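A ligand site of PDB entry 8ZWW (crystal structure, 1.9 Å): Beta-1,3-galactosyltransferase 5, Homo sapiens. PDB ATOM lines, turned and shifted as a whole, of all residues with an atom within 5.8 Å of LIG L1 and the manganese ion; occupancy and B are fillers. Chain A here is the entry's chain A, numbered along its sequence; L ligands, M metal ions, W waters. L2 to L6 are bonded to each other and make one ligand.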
ATOM      1  N   THR A  34      14.134  -4.763  12.547  1.00  0.00           N
ATOM      2  CA  THR A  34      15.219  -3.849  12.881  1.00  0.00           C
ATOM      3  C   THR A  34      16.113  -4.477  13.944  1.00  0.00           C
ATOM      4  O   THR A  34      15.631  -5.132  14.891  1.00  0.00           O
ATOM      5  CB  THR A  34      14.696  -2.501  13.389  1.00  0.00           C
ATOM      6  OG1 THR A  34      13.977  -2.715  14.603  1.00  0.00           O
ATOM      7  CG2 THR A  34      13.798  -1.833  12.357  1.00  0.00           C
ATOM      8  N   SER A  35      17.420  -4.275  13.791  1.00  0.00           N
ATOM      9  CA  SER A  35      18.398  -4.678  14.791  1.00  0.00           C
ATOM     10  C   SER A  35      19.693  -3.942  14.460  1.00  0.00           C
ATOM     11  O   SER A  35      19.910  -3.519  13.327  1.00  0.00           O
ATOM     12  CB  SER A  35      18.603  -6.197  14.823  1.00  0.00           C
ATOM     13  OG  SER A  35      19.191  -6.684  13.629  1.00  0.00           O
ATOM     14  N   SER A  36      20.543  -3.777  15.476  1.00  0.00           N
ATOM     15  CA  SER A  36      21.828  -3.133  15.252  1.00  0.00           C
ATOM     16  C   SER A  36      22.849  -4.162  14.753  1.00  0.00           C
ATOM     17  O   SER A  36      22.617  -5.370  14.769  1.00  0.00           O
ATOM     18  CB  SER A  36      22.302  -2.420  16.524  1.00  0.00           C
ATOM     19  OG  SER A  36      22.688  -3.342  17.515  1.00  0.00           O
ATOM     20  N   GLN A  39      23.852  -7.189  17.002  1.00  0.00           N
ATOM     21  CA  GLN A  39      22.808  -8.084  17.498  1.00  0.00           C
ATOM     22  C   GLN A  39      22.636  -9.292  16.582  1.00  0.00           C
ATOM     23  O   GLN A  39      21.511  -9.628  16.167  1.00  0.00           O
ATOM     24  CB  GLN A  39      21.502  -7.313  17.643  1.00  0.00           C
ATOM     25  CG  GLN A  39      21.560  -6.187  18.664  1.00  0.00           C
ATOM     26  CD  GLN A  39      20.248  -5.437  18.816  1.00  0.00           C
ATOM     27  OE1 GLN A  39      19.877  -4.648  17.946  1.00  0.00           O
ATOM     28  NE2 GLN A  39      19.566  -5.644  19.930  1.00  0.00           N
ATOM     29  N   LEU A  66      16.761  -5.204   8.430  1.00  0.00           N
ATOM     30  CA  LEU A  66      17.146  -3.856   8.024  1.00  0.00           C
ATOM     31  C   LEU A  66      18.409  -3.456   8.771  1.00  0.00           C
ATOM     32  O   LEU A  66      18.468  -3.522  10.006  1.00  0.00           O
ATOM     33  CB  LEU A  66      16.020  -2.873   8.320  1.00  0.00           C
ATOM     34  CG  LEU A  66      14.610  -3.226   7.843  1.00  0.00           C
ATOM     35  CD1 LEU A  66      13.618  -2.089   8.190  1.00  0.00           C
ATOM     36  CD2 LEU A  66      14.580  -3.472   6.340  1.00  0.00           C
ATOM     37  N   ASP A  96      23.985   3.555  11.467  1.00  0.00           N
ATOM     38  CA  ASP A  96      22.975   2.756  12.149  1.00  0.00           C
ATOM     39  C   ASP A  96      23.072   2.999  13.646  1.00  0.00           C
ATOM     40  O   ASP A  96      23.798   2.295  14.350  1.00  0.00           O
ATOM     41  CB  ASP A  96      23.140   1.286  11.810  1.00  0.00           C
ATOM     42  CG  ASP A  96      21.924   0.450  12.193  1.00  0.00           C
ATOM     43  OD1 ASP A  96      21.114   0.906  13.050  1.00  0.00           O
ATOM     44  OD2 ASP A  96      21.769  -0.653  11.642  1.00  0.00           O
ATOM     45  N   VAL A  97      22.353   4.006  14.131  1.00  0.00           N
ATOM     46  CA  VAL A  97      22.266   4.351  15.551  1.00  0.00           C
ATOM     47  C   VAL A  97      20.795   4.566  15.898  1.00  0.00           C
ATOM     48  O   VAL A  97      19.928   4.684  15.025  1.00  0.00           O
ATOM     49  CB  VAL A  97      23.083   5.614  15.896  1.00  0.00           C
ATOM     50  CG1 VAL A  97      24.570   5.372  15.731  1.00  0.00           C
ATOM     51  CG2 VAL A  97      22.626   6.779  15.048  1.00  0.00           C
ATOM     52  N   TYR A  98      20.504   4.571  17.205  1.00  0.00           N
ATOM     53  CA  TYR A  98      19.108   4.668  17.658  1.00  0.00           C
ATOM     54  C   TYR A  98      18.403   5.874  17.044  1.00  0.00           C
ATOM     55  O   TYR A  98      17.270   5.768  16.543  1.00  0.00           O
ATOM     56  CB  TYR A  98      19.045   4.738  19.189  1.00  0.00           C
ATOM     57  CG  TYR A  98      17.670   4.393  19.713  1.00  0.00           C
ATOM     58  CD1 TYR A  98      17.299   3.060  19.937  1.00  0.00           C
ATOM     59  CD2 TYR A  98      16.728   5.386  19.940  1.00  0.00           C
ATOM     60  CE1 TYR A  98      16.019   2.738  20.394  1.00  0.00           C
ATOM     61  CE2 TYR A  98      15.453   5.077  20.396  1.00  0.00           C
ATOM     62  CZ  TYR A  98      15.104   3.750  20.613  1.00  0.00           C
ATOM     63  OH  TYR A  98      13.853   3.477  21.065  1.00  0.00           O
ATOM     64  N   LEU A 101      16.788   5.588  13.551  1.00  0.00           N
ATOM     65  CA  LEU A 101      15.778   4.569  13.263  1.00  0.00           C
ATOM     66  C   LEU A 101      14.772   5.029  12.206  1.00  0.00           C
ATOM     67  O   LEU A 101      14.286   4.191  11.431  1.00  0.00           O
ATOM     68  CB  LEU A 101      15.068   4.162  14.560  1.00  0.00           C
ATOM     69  CG  LEU A 101      15.901   3.213  15.421  1.00  0.00           C
ATOM     70  CD1 LEU A 101      15.190   2.845  16.732  1.00  0.00           C
ATOM     71  CD2 LEU A 101      16.254   1.950  14.587  1.00  0.00           C
ATOM     72  N   LYS A 104      16.116   4.084   9.038  1.00  0.00           N
ATOM     73  CA  LYS A 104      16.030   2.639   8.871  1.00  0.00           C
ATOM     74  C   LYS A 104      14.626   2.246   8.440  1.00  0.00           C
ATOM     75  O   LYS A 104      14.444   1.483   7.472  1.00  0.00           O
ATOM     76  CB  LYS A 104      16.411   1.914  10.150  1.00  0.00           C
ATOM     77  CG  LYS A 104      16.366   0.407   9.971  1.00  0.00           C
ATOM     78  CD  LYS A 104      17.012  -0.333  11.153  1.00  0.00           C
ATOM     79  CE  LYS A 104      18.527  -0.189  11.113  1.00  0.00           C
ATOM     80  NZ  LYS A 104      19.198  -1.211  11.969  1.00  0.00           N
ATOM     81  N   LYS A 124       6.523  -4.139  10.133  1.00  0.00           N
ATOM     82  CA  LYS A 124       7.776  -3.631  10.668  1.00  0.00           C
ATOM     83  C   LYS A 124       7.845  -4.017  12.144  1.00  0.00           C
ATOM     84  O   LYS A 124       6.889  -3.772  12.899  1.00  0.00           O
ATOM     85  CB  LYS A 124       7.881  -2.116  10.474  1.00  0.00           C
ATOM     86  CG  LYS A 124       9.180  -1.497  11.061  1.00  0.00           C
ATOM     87  CD  LYS A 124       8.974  -1.005  12.530  1.00  0.00           C
ATOM     88  CE  LYS A 124      10.309  -0.680  13.219  1.00  0.00           C
ATOM     89  NZ  LYS A 124      10.198  -0.151  14.608  1.00  0.00           N
ATOM     90  N   THR A 125       8.937  -4.657  12.550  1.00  0.00           N
ATOM     91  CA  THR A 125       9.052  -5.131  13.924  1.00  0.00           C
ATOM     92  C   THR A 125      10.474  -4.942  14.440  1.00  0.00           C
ATOM     93  O   THR A 125      11.422  -4.682  13.688  1.00  0.00           O
ATOM     94  CB  THR A 125       8.602  -6.593  14.092  1.00  0.00           C
ATOM     95  OG1 THR A 125       8.662  -6.932  15.487  1.00  0.00           O
ATOM     96  CG2 THR A 125       9.482  -7.578  13.311  1.00  0.00           C
ATOM     97  N   ASP A 126      10.576  -4.993  15.753  1.00  0.00           N
ATOM     98  CA  ASP A 126      11.835  -4.942  16.464  1.00  0.00           C
ATOM     99  C   ASP A 126      12.333  -6.346  16.716  1.00  0.00           C
ATOM    100  O   ASP A 126      11.658  -7.345  16.445  1.00  0.00           O
ATOM    101  CB  ASP A 126      11.648  -4.142  17.739  1.00  0.00           C
ATOM    102  CG  ASP A 126      11.470  -2.660  17.449  1.00  0.00           C
ATOM    103  OD1 ASP A 126      11.656  -2.310  16.263  1.00  0.00           O
ATOM    104  OD2 ASP A 126      11.131  -1.866  18.338  1.00  0.00           O
ATOM    105  N   SER A 127      13.572  -6.434  17.205  1.00  0.00           N
ATOM    106  CA  SER A 127      14.224  -7.717  17.380  1.00  0.00           C
ATOM    107  C   SER A 127      14.027  -8.303  18.767  1.00  0.00           C
ATOM    108  O   SER A 127      14.327  -9.492  18.965  1.00  0.00           O
ATOM    109  CB  SER A 127      15.729  -7.581  17.057  1.00  0.00           C
ATOM    110  OG  SER A 127      16.301  -6.503  17.785  1.00  0.00           O
ATOM    111  N   ASP A 128      13.546  -7.512  19.731  1.00  0.00           N
ATOM    112  CA  ASP A 128      13.262  -8.011  21.083  1.00  0.00           C
ATOM    113  C   ASP A 128      11.806  -8.421  21.197  1.00  0.00           C
ATOM    114  O   ASP A 128      11.094  -8.011  22.123  1.00  0.00           O
ATOM    115  CB  ASP A 128      13.650  -6.955  22.110  1.00  0.00           C
ATOM    116  CG  ASP A 128      13.017  -5.590  21.831  1.00  0.00           C
ATOM    117  OD1 ASP A 128      12.461  -5.378  20.741  1.00  0.00           O
ATOM    118  OD2 ASP A 128      13.131  -4.687  22.686  1.00  0.00           O
ATOM    119  N   LYS A 167      15.152   8.368  27.059  1.00  0.00           N
ATOM    120  CA  LYS A 167      15.487   7.730  25.785  1.00  0.00           C
ATOM    121  C   LYS A 167      14.676   8.301  24.624  1.00  0.00           C
ATOM    122  O   LYS A 167      15.179   8.381  23.489  1.00  0.00           O
ATOM    123  CB  LYS A 167      15.263   6.223  25.898  1.00  0.00           C
ATOM    124  CG  LYS A 167      15.804   5.390  24.748  1.00  0.00           C
ATOM    125  CD  LYS A 167      15.512   3.896  24.954  1.00  0.00           C
ATOM    126  CE  LYS A 167      16.006   3.067  23.778  1.00  0.00           C
ATOM    127  NZ  LYS A 167      16.000   1.598  24.068  1.00  0.00           N
ATOM    128  N   TRP A 168      13.433   8.713  24.859  1.00  0.00           N
ATOM    129  CA  TRP A 168      12.598   9.211  23.782  1.00  0.00           C
ATOM    130  C   TRP A 168      12.282  10.700  23.915  1.00  0.00           C
ATOM    131  O   TRP A 168      11.251  11.178  23.429  1.00  0.00           O
ATOM    132  CB  TRP A 168      11.313   8.388  23.693  1.00  0.00           C
ATOM    133  CG  TRP A 168      11.615   6.921  23.662  1.00  0.00           C
ATOM    134  CD1 TRP A 168      12.027   6.187  22.580  1.00  0.00           C
ATOM    135  CD2 TRP A 168      11.503   6.016  24.756  1.00  0.00           C
ATOM    136  NE1 TRP A 168      12.189   4.865  22.947  1.00  0.00           N
ATOM    137  CE2 TRP A 168      11.879   4.734  24.280  1.00  0.00           C
ATOM    138  CE3 TRP A 168      11.128   6.154  26.095  1.00  0.00           C
ATOM    139  CZ2 TRP A 168      11.891   3.608  25.104  1.00  0.00           C
ATOM    140  CZ3 TRP A 168      11.148   5.032  26.908  1.00  0.00           C
ATOM    141  CH2 TRP A 168      11.523   3.773  26.413  1.00  0.00           C
ATOM    142  N   THR A 187       7.260  -1.162  18.263  1.00  0.00           N
ATOM    143  CA  THR A 187       7.649  -2.528  18.575  1.00  0.00           C
ATOM    144  C   THR A 187       7.185  -3.516  17.505  1.00  0.00           C
ATOM    145  O   THR A 187       7.833  -4.530  17.273  1.00  0.00           O
ATOM    146  CB  THR A 187       7.113  -2.965  19.941  1.00  0.00           C
ATOM    147  OG1 THR A 187       5.696  -2.783  19.958  1.00  0.00           O
ATOM    148  CG2 THR A 187       7.770  -2.151  21.066  1.00  0.00           C
ATOM    149  N   HIS A 255       6.494  -7.729  23.295  1.00  0.00           N
ATOM    150  CA  HIS A 255       7.764  -7.028  23.458  1.00  0.00           C
ATOM    151  C   HIS A 255       8.511  -7.542  24.685  1.00  0.00           C
ATOM    152  O   HIS A 255       8.020  -8.394  25.435  1.00  0.00           O
ATOM    153  CB  HIS A 255       7.468  -5.525  23.546  1.00  0.00           C
ATOM    154  CG  HIS A 255       8.675  -4.650  23.529  1.00  0.00           C
ATOM    155  ND1 HIS A 255       8.821  -3.562  24.368  1.00  0.00           N
ATOM    156  CD2 HIS A 255       9.766  -4.645  22.724  1.00  0.00           C
ATOM    157  CE1 HIS A 255       9.957  -2.944  24.101  1.00  0.00           C
ATOM    158  NE2 HIS A 255      10.557  -3.577  23.104  1.00  0.00           N
ATOM    159  N   PHE A 256       9.751  -7.073  24.856  1.00  0.00           N
ATOM    160  CA  PHE A 256      10.594  -7.390  26.018  1.00  0.00           C
ATOM    161  C   PHE A 256      11.020  -8.860  26.027  1.00  0.00           C
ATOM    162  O   PHE A 256      11.000  -9.506  27.068  1.00  0.00           O
ATOM    163  CB  PHE A 256       9.878  -7.056  27.344  1.00  0.00           C
ATOM    164  CG  PHE A 256       9.678  -5.558  27.562  1.00  0.00           C
ATOM    165  CD1 PHE A 256      10.744  -4.674  27.466  1.00  0.00           C
ATOM    166  CD2 PHE A 256       8.407  -5.035  27.817  1.00  0.00           C
ATOM    167  CE1 PHE A 256      10.565  -3.300  27.633  1.00  0.00           C
ATOM    168  CE2 PHE A 256       8.213  -3.670  27.989  1.00  0.00           C
ATOM    169  CZ  PHE A 256       9.297  -2.801  27.891  1.00  0.00           C
HETATM  170  N1  LIG L   1      17.983  -0.718  16.842  1.00  0.00           N
HETATM  171  C1  LIG L   1      18.662  -0.655  15.622  1.00  0.00           C
HETATM  172  N2  LIG L   1      19.799   0.119  15.642  1.00  0.00           N
HETATM  173  C2  LIG L   1      20.300   0.826  16.708  1.00  0.00           C
HETATM  174  C3  LIG L   1      19.542   0.726  17.916  1.00  0.00           C
HETATM  175  C4  LIG L   1      18.423  -0.032  17.945  1.00  0.00           C
HETATM  176  O1  LIG L   1      18.306  -1.252  14.620  1.00  0.00           O
HETATM  177  O2  LIG L   1      21.334   1.502  16.571  1.00  0.00           O
HETATM  178  C5  LIG L   1      16.768  -1.536  16.894  1.00  0.00           C
HETATM  179  C6  LIG L   1      16.729  -2.492  18.082  1.00  0.00           C
HETATM  180  O3  LIG L   1      17.397  -3.712  17.795  1.00  0.00           O
HETATM  181  C7  LIG L   1      15.223  -2.699  18.217  1.00  0.00           C
HETATM  182  C8  LIG L   1      14.662  -1.318  17.879  1.00  0.00           C
HETATM  183  O4  LIG L   1      15.667  -0.671  17.068  1.00  0.00           O
HETATM  184  O5  LIG L   1      14.824  -3.733  17.322  1.00  0.00           O
HETATM  185  C9  LIG L   1      14.384  -0.474  19.099  1.00  0.00           C
HETATM  186  O6  LIG L   1      15.438  -0.680  20.066  1.00  0.00           O
HETATM  187  P1  LIG L   1      15.136  -0.736  21.623  1.00  0.00           P
HETATM  188  O7  LIG L   1      16.400  -0.428  22.325  1.00  0.00           O
HETATM  189  O8  LIG L   1      14.432  -2.041  21.992  1.00  0.00           O
HETATM  190  O9  LIG L   1      14.087   0.437  21.846  1.00  0.00           O
HETATM  191  P2  LIG L   1      12.969   0.547  22.965  1.00  0.00           P
HETATM  192  O10 LIG L   1      12.436   1.973  22.770  1.00  0.00           O
HETATM  193  O11 LIG L   1      11.859  -0.450  22.475  1.00  0.00           O
HETATM  194  O12 LIG L   1      13.538   0.304  24.355  1.00  0.00           O
HETATM  195  C1  LG2 L   2      13.159   5.503  32.987  1.00  0.00           C
HETATM  196  C2  LG2 L   2      11.703   5.526  32.517  1.00  0.00           C
HETATM  197  C3  LG2 L   2      11.507   4.507  31.392  1.00  0.00           C
HETATM  198  C4  LG2 L   2      11.983   3.131  31.844  1.00  0.00           C
HETATM  199  C5  LG2 L   2      11.870   2.094  30.759  1.00  0.00           C
HETATM  200  C6  LG2 L   2      13.627   4.083  33.312  1.00  0.00           C
HETATM  201  O1  LG2 L   2      15.001   4.104  33.575  1.00  0.00           O
HETATM  202  O2  LG2 L   2      13.301   6.324  34.143  1.00  0.00           O
HETATM  203  O3  LG2 L   2      11.368   6.832  32.073  1.00  0.00           O
HETATM  204  O4  LG2 L   2      10.166   4.386  30.937  1.00  0.00           O
HETATM  205  O5  LG2 L   2      13.368   3.210  32.204  1.00  0.00           O
HETATM  206  O6  LG2 L   2      12.931   2.238  29.825  1.00  0.00           O
HETATM  207  C1  LG3 L   3       9.053   5.236  31.323  1.00  0.00           C
HETATM  208  C2  LG3 L   3       8.799   6.226  30.256  1.00  0.00           C
HETATM  209  C3  LG3 L   3       7.419   6.912  30.396  1.00  0.00           C
HETATM  210  C4  LG3 L   3       6.373   5.774  30.352  1.00  0.00           C
HETATM  211  C5  LG3 L   3       6.637   4.866  31.544  1.00  0.00           C
HETATM  212  C6  LG3 L   3       5.739   3.603  31.644  1.00  0.00           C
HETATM  213  O1  LG3 L   3       9.773   7.292  30.233  1.00  0.00           O
HETATM  214  O2  LG3 L   3       7.167   7.811  29.360  1.00  0.00           O
HETATM  215  O3  LG3 L   3       6.550   5.062  29.133  1.00  0.00           O
HETATM  216  O4  LG3 L   3       7.983   4.331  31.503  1.00  0.00           O
HETATM  217  O5  LG3 L   3       6.232   2.566  30.839  1.00  0.00           O
HETATM  218  C1  LG4 L   4       5.315   4.850  28.434  1.00  0.00           C
HETATM  219  C2  LG4 L   4       5.684   4.174  27.116  1.00  0.00           C
HETATM  220  C3  LG4 L   4       6.220   5.156  26.104  1.00  0.00           C
HETATM  221  C4  LG4 L   4       5.262   6.293  25.857  1.00  0.00           C
HETATM  222  C5  LG4 L   4       5.036   7.004  27.197  1.00  0.00           C
HETATM  223  C6  LG4 L   4       4.065   8.140  27.072  1.00  0.00           C
HETATM  224  O1  LG4 L   4       6.694   3.176  27.355  1.00  0.00           O
HETATM  225  O2  LG4 L   4       6.460   4.404  24.899  1.00  0.00           O
HETATM  226  O3  LG4 L   4       4.056   5.828  25.309  1.00  0.00           O
HETATM  227  O4  LG4 L   4       4.514   6.092  28.230  1.00  0.00           O
HETATM  228  O5  LG4 L   4       3.481   8.337  28.345  1.00  0.00           O
HETATM  229  C1  LG5 L   5       7.472   4.994  24.053  1.00  0.00           C
HETATM  230  C2  LG5 L   5       7.859   3.868  23.101  1.00  0.00           C
HETATM  231  C3  LG5 L   5       8.734   4.356  21.957  1.00  0.00           C
HETATM  232  C4  LG5 L   5       8.158   5.634  21.378  1.00  0.00           C
HETATM  233  C5  LG5 L   5       7.885   6.679  22.463  1.00  0.00           C
HETATM  234  C6  LG5 L   5       7.373   7.999  21.886  1.00  0.00           C
HETATM  235  C7  LG5 L   5       8.150   1.575  23.963  1.00  0.00           C
HETATM  236  C8  LG5 L   5       9.212   0.558  24.301  1.00  0.00           C
HETATM  237  N1  LG5 L   5       8.606   2.829  23.784  1.00  0.00           N
HETATM  238  O1  LG5 L   5       8.726   3.296  21.010  1.00  0.00           O
HETATM  239  O2  LG5 L   5       6.944   5.277  20.772  1.00  0.00           O
HETATM  240  O3  LG5 L   5       6.959   6.116  23.369  1.00  0.00           O
HETATM  241  O4  LG5 L   5       7.231   8.968  22.913  1.00  0.00           O
HETATM  242  O5  LG5 L   5       6.967   1.236  23.850  1.00  0.00           O
HETATM  243  C1  LG6 L   6       9.972   3.126  20.308  1.00  0.00           C
HETATM  244  C2  LG6 L   6       9.815   1.837  19.466  1.00  0.00           C
HETATM  245  C3  LG6 L   6      10.966   1.670  18.463  1.00  0.00           C
HETATM  246  C4  LG6 L   6      11.063   2.928  17.607  1.00  0.00           C
HETATM  247  C5  LG6 L   6      11.324   4.116  18.529  1.00  0.00           C
HETATM  248  C6  LG6 L   6      11.477   5.490  17.790  1.00  0.00           C
HETATM  249  O1  LG6 L   6       9.783   0.622  20.248  1.00  0.00           O
HETATM  250  O2  LG6 L   6      10.702   0.545  17.629  1.00  0.00           O
HETATM  251  O3  LG6 L   6       9.835   3.161  16.918  1.00  0.00           O
HETATM  252  O4  LG6 L   6      10.273   4.273  19.503  1.00  0.00           O
HETATM  253  O5  LG6 L   6      12.504   5.464  16.829  1.00  0.00           O
HETATM  254 MN    MN M   1      12.395  -2.596  22.421  1.00  0.00          MN
HETATM  255  O   HOH W   1      18.839  -2.613  20.686  1.00  0.00           O
HETATM  256  O   HOH W   2      18.609  -0.203  21.131  1.00  0.00           O
HETATM  257  O   HOH W   3      11.558  -2.833  20.483  1.00  0.00           O
HETATM  258  O   HOH W   4      13.466  -2.250  24.679  1.00  0.00           O
HETATM  259  O   HOH W   5      16.170  -3.731  21.697  1.00  0.00           O
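An oxygen (O3) of LIG L1 lies within hydrogen-bond range of the side-chain amide oxygen (OE1) of Gln 39 (2.7 Å). The backbone NH of Tyr 98 is in hydrogen-bond range of an oxygen (O2) of LIG L1. The side-chain hydroxyl (OH) of Tyr 98 is in hydrogen-bond range of an oxygen (O10) of LIG L1 (2.7 Å). O7 of LIG L1 lies within salt-bridge range of NZ of Lys 167 (2.7 Å). The side-chain amino group of Lys 104 sits at hydrogen-bond distance from an oxygen (O1) of LIG L1, 2.8 Å away. An oxygen (O10) of LIG L1 sits close to the indole nitrogen (NE1) of Trp 168 (2.9 Å). O5 of LIG L1 sits at hydrogen-bond distance from O of Thr 34. An oxygen (O5) of LIG L1 is in hydrogen-bond range of the side-chain hydroxyl of Thr 34, at 3.0 Å. N of Ser 127 is in hydrogen-bond range of O5 of LIG L1, 3.0 Å away. The side-chain hydroxyl (OG) of Ser 127 is in hydrogen-bond range of an oxygen (O3) of LIG L1. The side-chain carboxylate (OD1) of Asp 96 sits at hydrogen-bond distance from a nitrogen (N2) of LIG L1, at 3.0 Å. An oxygen (O1) of LIG L1 sits close to the backbone NH (N) of Ser 35, at 3.3 Å. N of Ser 36 sits at hydrogen-bond distance from O1 of LIG L1. OD2 of Asp 126 lies within hydrogen-bond range of O2 of LG6 L6. An oxygen (O2) of LG6 L6 is in hydrogen-bond range of the side-chain amino group of Lys 124, at 3.1 Å.
An oxygen (O11) of LIG L1 sits close to an oxygen (O1) of LG6 L6.
Water W3 binds the manganese ion, at 2.1 Å. The manganese ion is bound by O8 of LIG L1 (2.2 Å). A ring nitrogen (NE2) of His 255 is bound to the manganese ion, at 2.2 Å. O11 of LIG L1 is bound to the manganese ion, 2.2 Å away. The side-chain carboxylate (OD2) of Asp 128 is bound to the manganese ion. Water W4 is bound to the manganese ion (2.5 Å). The manganese ion has six donor atoms within binding distance.
CA of Val 97 touches O2 of LIG L1, 3.2 Å away. Leu 101 touches LIG L1. Asp 126 touches LIG L1 (CB to O5, 3.2 Å). 15 residues have an atom within 4 Å of LIG L1: Thr 34, Ser 35, Ser 36, Gln 39, Asp 96, Val 97, Tyr 98, Leu 101, Lys 104, Asp 126, Ser 127, Asp 128, Lys 167, Trp 168 and His 255.
Within 4 Å of the manganese ion: Asp 128 and His 255. The nearest printed residue that does not touch the manganese ion is Asp 126 (4.3 Å).
Water W1 bridges NE2 of Gln 39 and O3 of LIG L1.
O of Asp 128 sits at hydrogen-bond distance from N of Phe 256, 3.2 Å away. The backbone NH of Ser 36 lies within hydrogen-bond range of the side-chain amide oxygen of Gln 39. The side-chain hydroxyl of Tyr 98 lies within hydrogen-bond range of the indole nitrogen of Trp 168, 2.9 Å away. The side-chain amino group (NZ) of Lys 104 lies within hydrogen-bond range of the backbone carbonyl oxygen (O) of Leu 66 (3.1 Å). The side-chain hydroxyl (OG) of Ser 127 sits close to the backbone carbonyl oxygen (O) of Thr 34, 3.3 Å away. The side-chain hydroxyl of Thr 34 is in hydrogen-bond range of the side-chain carboxylate of Asp 126. The backbone NH of Thr 34 sits at hydrogen-bond distance from the backbone carbonyl oxygen of Thr 125. The side-chain carboxylate (OD1) of Asp 126 lies within salt-bridge range of the side-chain amino group (NZ) of Lys 124, 3.1 Å away.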
